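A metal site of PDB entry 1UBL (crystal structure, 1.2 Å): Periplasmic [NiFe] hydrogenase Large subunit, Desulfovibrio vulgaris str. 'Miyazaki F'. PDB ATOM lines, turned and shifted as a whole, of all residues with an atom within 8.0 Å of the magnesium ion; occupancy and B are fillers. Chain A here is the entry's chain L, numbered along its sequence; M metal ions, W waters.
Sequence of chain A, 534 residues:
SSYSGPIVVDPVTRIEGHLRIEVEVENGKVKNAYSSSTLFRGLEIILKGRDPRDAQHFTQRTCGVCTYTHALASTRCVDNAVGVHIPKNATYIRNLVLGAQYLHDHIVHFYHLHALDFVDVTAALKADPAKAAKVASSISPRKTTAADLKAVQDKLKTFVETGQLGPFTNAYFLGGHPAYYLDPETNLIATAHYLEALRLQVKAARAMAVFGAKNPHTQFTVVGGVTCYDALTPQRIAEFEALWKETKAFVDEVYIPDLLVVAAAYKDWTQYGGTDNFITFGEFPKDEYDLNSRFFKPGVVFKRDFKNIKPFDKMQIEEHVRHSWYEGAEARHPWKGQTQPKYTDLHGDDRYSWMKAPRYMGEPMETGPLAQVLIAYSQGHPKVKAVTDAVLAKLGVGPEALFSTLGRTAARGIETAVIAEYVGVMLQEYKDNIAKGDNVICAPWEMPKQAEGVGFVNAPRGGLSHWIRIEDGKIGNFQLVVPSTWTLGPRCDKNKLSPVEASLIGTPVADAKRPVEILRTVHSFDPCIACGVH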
ATOM      1  N   PHE A  40      15.241  16.603  30.105  1.00  0.00           N
ATOM      2  CA  PHE A  40      14.967  15.441  29.292  1.00  0.00           C
ATOM      3  C   PHE A  40      13.769  15.722  28.365  1.00  0.00           C
ATOM      4  O   PHE A  40      12.775  16.330  28.793  1.00  0.00           O
ATOM      5  CB  PHE A  40      14.678  14.235  30.180  1.00  0.00           C
ATOM      6  CG  PHE A  40      14.208  12.980  29.480  1.00  0.00           C
ATOM      7  CD1 PHE A  40      15.166  12.156  28.895  1.00  0.00           C
ATOM      8  CD2 PHE A  40      12.869  12.657  29.366  1.00  0.00           C
ATOM      9  CE1 PHE A  40      14.790  10.974  28.231  1.00  0.00           C
ATOM     10  CE2 PHE A  40      12.463  11.468  28.735  1.00  0.00           C
ATOM     11  CZ  PHE A  40      13.445  10.663  28.189  1.00  0.00           C
ATOM     12  N   GLU A  44      13.732   9.605  21.581  1.00  0.00           N
ATOM     13  CA  GLU A  44      13.787   8.163  21.226  1.00  0.00           C
ATOM     14  C   GLU A  44      12.462   7.476  21.549  1.00  0.00           C
ATOM     15  O   GLU A  44      12.029   6.583  20.803  1.00  0.00           O
ATOM     16  CB  GLU A  44      14.926   7.480  21.939  1.00  0.00           C
ATOM     17  CG  GLU A  44      16.311   7.970  21.480  1.00  0.00           C
ATOM     18  CD  GLU A  44      17.388   7.831  22.536  1.00  0.00           C
ATOM     19  OE1 GLU A  44      17.035   7.797  23.777  1.00  0.00           O
ATOM     20  OE2 GLU A  44      18.591   7.841  22.153  1.00  0.00           O
ATOM     21  N   GLU A 319      26.044   2.160  26.335  1.00  0.00           N
ATOM     22  CA  GLU A 319      25.606   3.339  27.079  1.00  0.00           C
ATOM     23  C   GLU A 319      25.105   2.915  28.466  1.00  0.00           C
ATOM     24  O   GLU A 319      24.165   2.147  28.615  1.00  0.00           O
ATOM     25  CB  GLU A 319      24.483   4.135  26.369  1.00  0.00           C
ATOM     26  CG  GLU A 319      24.994   4.711  25.044  1.00  0.00           C
ATOM     27  CD  GLU A 319      23.862   5.588  24.507  1.00  0.00           C
ATOM     28  OE1 GLU A 319      23.996   6.810  24.635  1.00  0.00           O
ATOM     29  OE2 GLU A 319      22.867   4.992  23.997  1.00  0.00           O
ATOM     30  N   TYR A 326      17.572   6.782  34.676  1.00  0.00           N
ATOM     31  CA  TYR A 326      16.894   5.753  33.868  1.00  0.00           C
ATOM     32  C   TYR A 326      16.777   4.517  34.749  1.00  0.00           C
ATOM     33  O   TYR A 326      17.464   4.395  35.785  1.00  0.00           O
ATOM     34  CB  TYR A 326      17.631   5.421  32.540  1.00  0.00           C
ATOM     35  CG  TYR A 326      17.690   6.659  31.679  1.00  0.00           C
ATOM     36  CD1 TYR A 326      18.867   7.417  31.695  1.00  0.00           C
ATOM     37  CD2 TYR A 326      16.583   7.029  30.914  1.00  0.00           C
ATOM     38  CE1 TYR A 326      18.925   8.558  30.917  1.00  0.00           C
ATOM     39  CE2 TYR A 326      16.674   8.208  30.145  1.00  0.00           C
ATOM     40  CZ  TYR A 326      17.831   8.935  30.160  1.00  0.00           C
ATOM     41  OH  TYR A 326      17.867  10.077  29.393  1.00  0.00           O
ATOM     42  N   PRO A 334      23.663   0.404  21.452  1.00  0.00           N
ATOM     43  CA  PRO A 334      22.463   1.146  20.957  1.00  0.00           C
ATOM     44  C   PRO A 334      21.511   0.366  20.053  1.00  0.00           C
ATOM     45  O   PRO A 334      20.346   0.744  20.025  1.00  0.00           O
ATOM     46  CB  PRO A 334      23.055   2.352  20.217  1.00  0.00           C
ATOM     47  CG  PRO A 334      24.509   2.276  20.374  1.00  0.00           C
ATOM     48  CD  PRO A 334      24.919   1.067  21.103  1.00  0.00           C
ATOM     49  N   GLY A 337      19.262  -0.614  22.576  1.00  0.00           N
ATOM     50  CA  GLY A 337      19.146   0.454  23.566  1.00  0.00           C
ATOM     51  C   GLY A 337      17.797   0.547  24.241  1.00  0.00           C
ATOM     52  O   GLY A 337      16.791   0.018  23.747  1.00  0.00           O
ATOM     53  N   GLN A 338      17.779   1.214  25.402  1.00  0.00           N
ATOM     54  CA  GLN A 338      16.595   1.379  26.222  1.00  0.00           C
ATOM     55  C   GLN A 338      16.558   2.802  26.739  1.00  0.00           C
ATOM     56  O   GLN A 338      17.591   3.305  27.177  1.00  0.00           O
ATOM     57  CB  GLN A 338      16.565   0.466  27.470  1.00  0.00           C
ATOM     58  CG  GLN A 338      16.521  -1.015  27.044  1.00  0.00           C
ATOM     59  CD  GLN A 338      16.475  -1.887  28.292  1.00  0.00           C
ATOM     60  OE1 GLN A 338      15.557  -2.686  28.461  1.00  0.00           O
ATOM     61  NE2 GLN A 338      17.471  -1.697  29.166  1.00  0.00           N
ATOM     62  N   THR A 339      15.389   3.425  26.707  1.00  0.00           N
ATOM     63  CA  THR A 339      15.261   4.822  27.225  1.00  0.00           C
ATOM     64  C   THR A 339      14.044   4.818  28.126  1.00  0.00           C
ATOM     65  O   THR A 339      12.907   5.039  27.690  1.00  0.00           O
ATOM     66  CB  THR A 339      15.153   5.828  26.067  1.00  0.00           C
ATOM     67  OG1 THR A 339      16.310   5.600  25.264  1.00  0.00           O
ATOM     68  CG2 THR A 339      15.129   7.249  26.602  1.00  0.00           C
ATOM     69  N   TRP A 354      20.414  13.398  33.286  1.00  0.00           N
ATOM     70  CA  TRP A 354      19.576  12.798  32.244  1.00  0.00           C
ATOM     71  C   TRP A 354      20.417  12.272  31.093  1.00  0.00           C
ATOM     72  O   TRP A 354      19.834  11.617  30.192  1.00  0.00           O
ATOM     73  CB  TRP A 354      18.559  13.810  31.713  1.00  0.00           C
ATOM     74  CG  TRP A 354      17.411  14.067  32.658  1.00  0.00           C
ATOM     75  CD1 TRP A 354      17.155  15.230  33.339  1.00  0.00           C
ATOM     76  CD2 TRP A 354      16.370  13.159  33.035  1.00  0.00           C
ATOM     77  NE1 TRP A 354      16.020  15.133  34.128  1.00  0.00           N
ATOM     78  CE2 TRP A 354      15.502  13.843  33.954  1.00  0.00           C
ATOM     79  CE3 TRP A 354      16.086  11.834  32.681  1.00  0.00           C
ATOM     80  CZ2 TRP A 354      14.364  13.221  34.516  1.00  0.00           C
ATOM     81  CZ3 TRP A 354      14.963  11.215  33.227  1.00  0.00           C
ATOM     82  CH2 TRP A 354      14.130  11.924  34.140  1.00  0.00           C
ATOM     83  N   MET A 355      21.735  12.536  31.036  1.00  0.00           N
ATOM     84  CA  MET A 355      22.518  11.863  29.997  1.00  0.00           C
ATOM     85  C   MET A 355      22.841  10.439  30.378  1.00  0.00           C
ATOM     86  O   MET A 355      23.150  10.170  31.547  1.00  0.00           O
ATOM     87  CB  MET A 355      23.843  12.592  29.746  1.00  0.00           C
ATOM     88  CG  MET A 355      23.684  13.908  29.010  1.00  0.00           C
ATOM     89  SD  MET A 355      25.321  14.408  28.386  1.00  0.00           S
ATOM     90  CE  MET A 355      25.045  16.178  28.132  1.00  0.00           C
ATOM     91  N   LYS A 356      22.842   9.530  29.415  1.00  0.00           N
ATOM     92  CA  LYS A 356      23.495   8.235  29.563  1.00  0.00           C
ATOM     93  C   LYS A 356      24.992   8.434  29.535  1.00  0.00           C
ATOM     94  O   LYS A 356      25.482   9.526  29.209  1.00  0.00           O
ATOM     95  CB  LYS A 356      23.046   7.287  28.460  1.00  0.00           C
ATOM     96  CG  LYS A 356      21.521   7.028  28.417  1.00  0.00           C
ATOM     97  CD  LYS A 356      21.153   6.134  27.240  1.00  0.00           C
ATOM     98  CE  LYS A 356      19.632   5.888  27.240  1.00  0.00           C
ATOM     99  NZ  LYS A 356      19.226   5.262  25.920  1.00  0.00           N
ATOM    100  N   PRO A 358      28.096   6.892  27.715  1.00  0.00           N
ATOM    101  CA  PRO A 358      28.660   5.994  26.705  1.00  0.00           C
ATOM    102  C   PRO A 358      30.098   5.648  27.072  1.00  0.00           C
ATOM    103  O   PRO A 358      30.859   6.500  27.513  1.00  0.00           O
ATOM    104  CB  PRO A 358      28.625   6.809  25.419  1.00  0.00           C
ATOM    105  CG  PRO A 358      27.701   7.969  25.701  1.00  0.00           C
ATOM    106  CD  PRO A 358      27.920   8.254  27.185  1.00  0.00           C
ATOM    107  N   SER A 465      26.194   9.207  16.297  1.00  0.00           N
ATOM    108  CA  SER A 465      25.677   7.982  15.647  1.00  0.00           C
ATOM    109  C   SER A 465      24.191   7.870  15.972  1.00  0.00           C
ATOM    110  O   SER A 465      23.764   8.084  17.099  1.00  0.00           O
ATOM    111  CB  SER A 465      26.534   6.728  15.990  1.00  0.00           C
ATOM    112  OG  SER A 465      26.609   6.525  17.421  1.00  0.00           O
ATOM    113  N   TRP A 467      21.031   5.027  15.332  1.00  0.00           N
ATOM    114  CA  TRP A 467      20.922   3.555  15.215  1.00  0.00           C
ATOM    115  C   TRP A 467      19.455   3.179  15.125  1.00  0.00           C
ATOM    116  O   TRP A 467      18.696   3.509  16.041  1.00  0.00           O
ATOM    117  CB  TRP A 467      21.495   2.926  16.489  1.00  0.00           C
ATOM    118  CG  TRP A 467      22.924   3.305  16.812  1.00  0.00           C
ATOM    119  CD1 TRP A 467      23.364   4.473  17.383  1.00  0.00           C
ATOM    120  CD2 TRP A 467      24.097   2.488  16.599  1.00  0.00           C
ATOM    121  NE1 TRP A 467      24.761   4.422  17.523  1.00  0.00           N
ATOM    122  CE2 TRP A 467      25.232   3.209  17.058  1.00  0.00           C
ATOM    123  CE3 TRP A 467      24.298   1.199  16.081  1.00  0.00           C
ATOM    124  CZ2 TRP A 467      26.510   2.683  16.978  1.00  0.00           C
ATOM    125  CZ3 TRP A 467      25.576   0.679  16.008  1.00  0.00           C
ATOM    126  CH2 TRP A 467      26.682   1.409  16.455  1.00  0.00           C
ATOM    127  N   PHE A 478      14.964   3.284  17.967  1.00  0.00           N
ATOM    128  CA  PHE A 478      15.801   4.308  17.380  1.00  0.00           C
ATOM    129  C   PHE A 478      16.604   4.906  18.519  1.00  0.00           C
ATOM    130  O   PHE A 478      16.026   5.352  19.525  1.00  0.00           O
ATOM    131  CB  PHE A 478      14.976   5.392  16.686  1.00  0.00           C
ATOM    132  CG  PHE A 478      15.803   6.195  15.667  1.00  0.00           C
ATOM    133  CD1 PHE A 478      16.723   7.152  16.107  1.00  0.00           C
ATOM    134  CD2 PHE A 478      15.630   5.974  14.308  1.00  0.00           C
ATOM    135  CE1 PHE A 478      17.494   7.841  15.152  1.00  0.00           C
ATOM    136  CE2 PHE A 478      16.377   6.668  13.389  1.00  0.00           C
ATOM    137  CZ  PHE A 478      17.343   7.601  13.786  1.00  0.00           C
ATOM    138  N   GLN A 479      17.932   4.885  18.408  1.00  0.00           N
ATOM    139  CA  GLN A 479      18.778   5.369  19.524  1.00  0.00           C
ATOM    140  C   GLN A 479      19.778   6.362  18.959  1.00  0.00           C
ATOM    141  O   GLN A 479      20.446   6.109  17.969  1.00  0.00           O
ATOM    142  CB  GLN A 479      19.493   4.222  20.212  1.00  0.00           C
ATOM    143  CG  GLN A 479      18.551   3.264  20.933  1.00  0.00           C
ATOM    144  CD  GLN A 479      17.956   3.835  22.195  1.00  0.00           C
ATOM    145  OE1 GLN A 479      18.616   4.636  22.903  1.00  0.00           O
ATOM    146  NE2 GLN A 479      16.734   3.465  22.567  1.00  0.00           N
ATOM    147  N   LEU A 480      19.885   7.498  19.652  1.00  0.00           N
ATOM    148  CA  LEU A 480      20.901   8.507  19.355  1.00  0.00           C
ATOM    149  C   LEU A 480      22.014   8.404  20.379  1.00  0.00           C
ATOM    150  O   LEU A 480      21.716   8.356  21.556  1.00  0.00           O
ATOM    151  CB  LEU A 480      20.380   9.952  19.371  1.00  0.00           C
ATOM    152  CG  LEU A 480      19.286  10.351  18.394  1.00  0.00           C
ATOM    153  CD1 LEU A 480      17.935   9.749  18.642  1.00  0.00           C
ATOM    154  CD2 LEU A 480      19.167  11.875  18.389  1.00  0.00           C
ATOM    155  N   VAL A 481      23.265   8.385  19.946  1.00  0.00           N
ATOM    156  CA  VAL A 481      24.407   8.427  20.856  1.00  0.00           C
ATOM    157  C   VAL A 481      25.221   9.644  20.372  1.00  0.00           C
ATOM    158  O   VAL A 481      25.713   9.621  19.217  1.00  0.00           O
ATOM    159  CB  VAL A 481      25.260   7.176  20.841  1.00  0.00           C
ATOM    160  CG1 VAL A 481      26.360   7.280  21.912  1.00  0.00           C
ATOM    161  CG2 VAL A 481      24.424   5.943  21.027  1.00  0.00           C
ATOM    162  N   VAL A 482      25.253  10.718  21.161  1.00  0.00           N
ATOM    163  CA  VAL A 482      25.607  12.034  20.596  1.00  0.00           C
ATOM    164  C   VAL A 482      26.937  12.491  21.184  1.00  0.00           C
ATOM    165  O   VAL A 482      27.322  12.042  22.286  1.00  0.00           O
ATOM    166  CB  VAL A 482      24.430  12.982  20.890  1.00  0.00           C
ATOM    167  CG1 VAL A 482      24.533  14.339  20.241  1.00  0.00           C
ATOM    168  CG2 VAL A 482      23.146  12.367  20.365  1.00  0.00           C
ATOM    169  N   THR A 485      27.019  13.454  24.740  1.00  0.00           N
ATOM    170  CA  THR A 485      26.755  12.325  25.624  1.00  0.00           C
ATOM    171  C   THR A 485      28.083  11.669  26.048  1.00  0.00           C
ATOM    172  O   THR A 485      28.334  11.394  27.230  1.00  0.00           O
ATOM    173  CB  THR A 485      25.864  11.278  24.924  1.00  0.00           C
ATOM    174  OG1 THR A 485      24.850  11.878  24.110  1.00  0.00           O
ATOM    175  CG2 THR A 485      25.205  10.423  26.014  1.00  0.00           C
ATOM    176  N   CYS A 531      21.524  18.011  22.669  1.00  0.00           N
ATOM    177  CA  CYS A 531      22.220  16.929  22.028  1.00  0.00           C
ATOM    178  C   CYS A 531      22.472  15.777  22.952  1.00  0.00           C
ATOM    179  O   CYS A 531      22.170  14.620  22.655  1.00  0.00           O
ATOM    180  CB  CYS A 531      23.566  17.411  21.430  1.00  0.00           C
ATOM    181  SG  CYS A 531      23.414  17.983  19.736  1.00  0.00           S
ATOM    182  N   GLY A 532      23.068  16.045  24.127  1.00  0.00           N
ATOM    183  CA  GLY A 532      23.532  14.939  24.930  1.00  0.00           C
ATOM    184  C   GLY A 532      22.394  14.065  25.460  1.00  0.00           C
ATOM    185  O   GLY A 532      22.576  12.855  25.583  1.00  0.00           O
ATOM    186  N   VAL A 533      21.258  14.659  25.801  1.00  0.00           N
ATOM    187  CA  VAL A 533      20.142  13.971  26.388  1.00  0.00           C
ATOM    188  C   VAL A 533      19.041  13.587  25.427  1.00  0.00           C
ATOM    189  O   VAL A 533      18.528  12.448  25.485  1.00  0.00           O
ATOM    190  CB  VAL A 533      19.440  14.826  27.482  1.00  0.00           C
ATOM    191  CG1 VAL A 533      18.249  14.082  28.061  1.00  0.00           C
ATOM    192  CG2 VAL A 533      20.388  15.225  28.595  1.00  0.00           C
ATOM    193  N   HIS A 534      18.670  14.446  24.457  1.00  0.00           N
ATOM    194  CA  HIS A 534      17.593  14.234  23.539  1.00  0.00           C
ATOM    195  C   HIS A 534      16.341  13.694  24.261  1.00  0.00           C
ATOM    196  O   HIS A 534      15.973  14.242  25.345  1.00  0.00           O
ATOM    197  CB  HIS A 534      18.035  13.425  22.285  1.00  0.00           C
ATOM    198  CG  HIS A 534      18.958  12.296  22.525  1.00  0.00           C
ATOM    199  ND1 HIS A 534      20.307  12.493  22.793  1.00  0.00           N
ATOM    200  CD2 HIS A 534      18.779  10.967  22.710  1.00  0.00           C
ATOM    201  CE1 HIS A 534      20.902  11.333  23.055  1.00  0.00           C
ATOM    202  NE2 HIS A 534      19.984  10.385  23.004  1.00  0.00           N
ATOM    203  OXT HIS A 534      15.690  12.755  23.735  1.00  0.00           O
HETATM  204 MG    MG M   1      20.404   8.274  23.259  1.00  0.00          MG
HETATM  205  O   HOH W   1      19.317   8.144  25.038  1.00  0.00           O
HETATM  206  O   HOH W   2      22.152   8.677  24.404  1.00  0.00           O
HETATM  207  O   HOH W   3      20.692   6.253  23.411  1.00  0.00           O
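A ring nitrogen (ND1) of His 534 sits at hydrogen-bond distance from the backbone carbonyl oxygen (O) of Cys 531, 2.8 Å away. The side-chain carboxylate of Glu 44 sits close to the side-chain amide oxygen of Gln 479 (3.3 Å). The side-chain carboxylate (OE1) of Glu 44 is in salt-bridge range of the side-chain amino group (NZ) of Lys 356 (3.98 Å). The side-chain carboxylate of Glu 44 is in hydrogen-bond range of the side-chain hydroxyl of Thr 339, at 2.8 Å.
Three residues have an atom within 4 Å of the magnesium ion: Glu 44, Leu 480 and His 534. The nearest printed residue that does not touch the magnesium ion is Gln 479 (4.1 Å).
The magnesium ion is bound by water W3 (2.0 Å), water W1 (2.1 Å), water W2 (2.1 Å), O of Leu 480 (2.2 Å), NE2 of His 534 (2.2 Å) and OE2 of Glu 44 (2.2 Å).
Water W1 lies within hydrogen-bond range of the side-chain carboxylate of Glu 44 and the side-chain amino group of Lys 356. Water W3 lies within hydrogen-bond range of OE2 of Glu 319 (2.6 Å), OE1 of Gln 479 (2.7 Å) and NZ of Lys 356 (3.1 Å).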
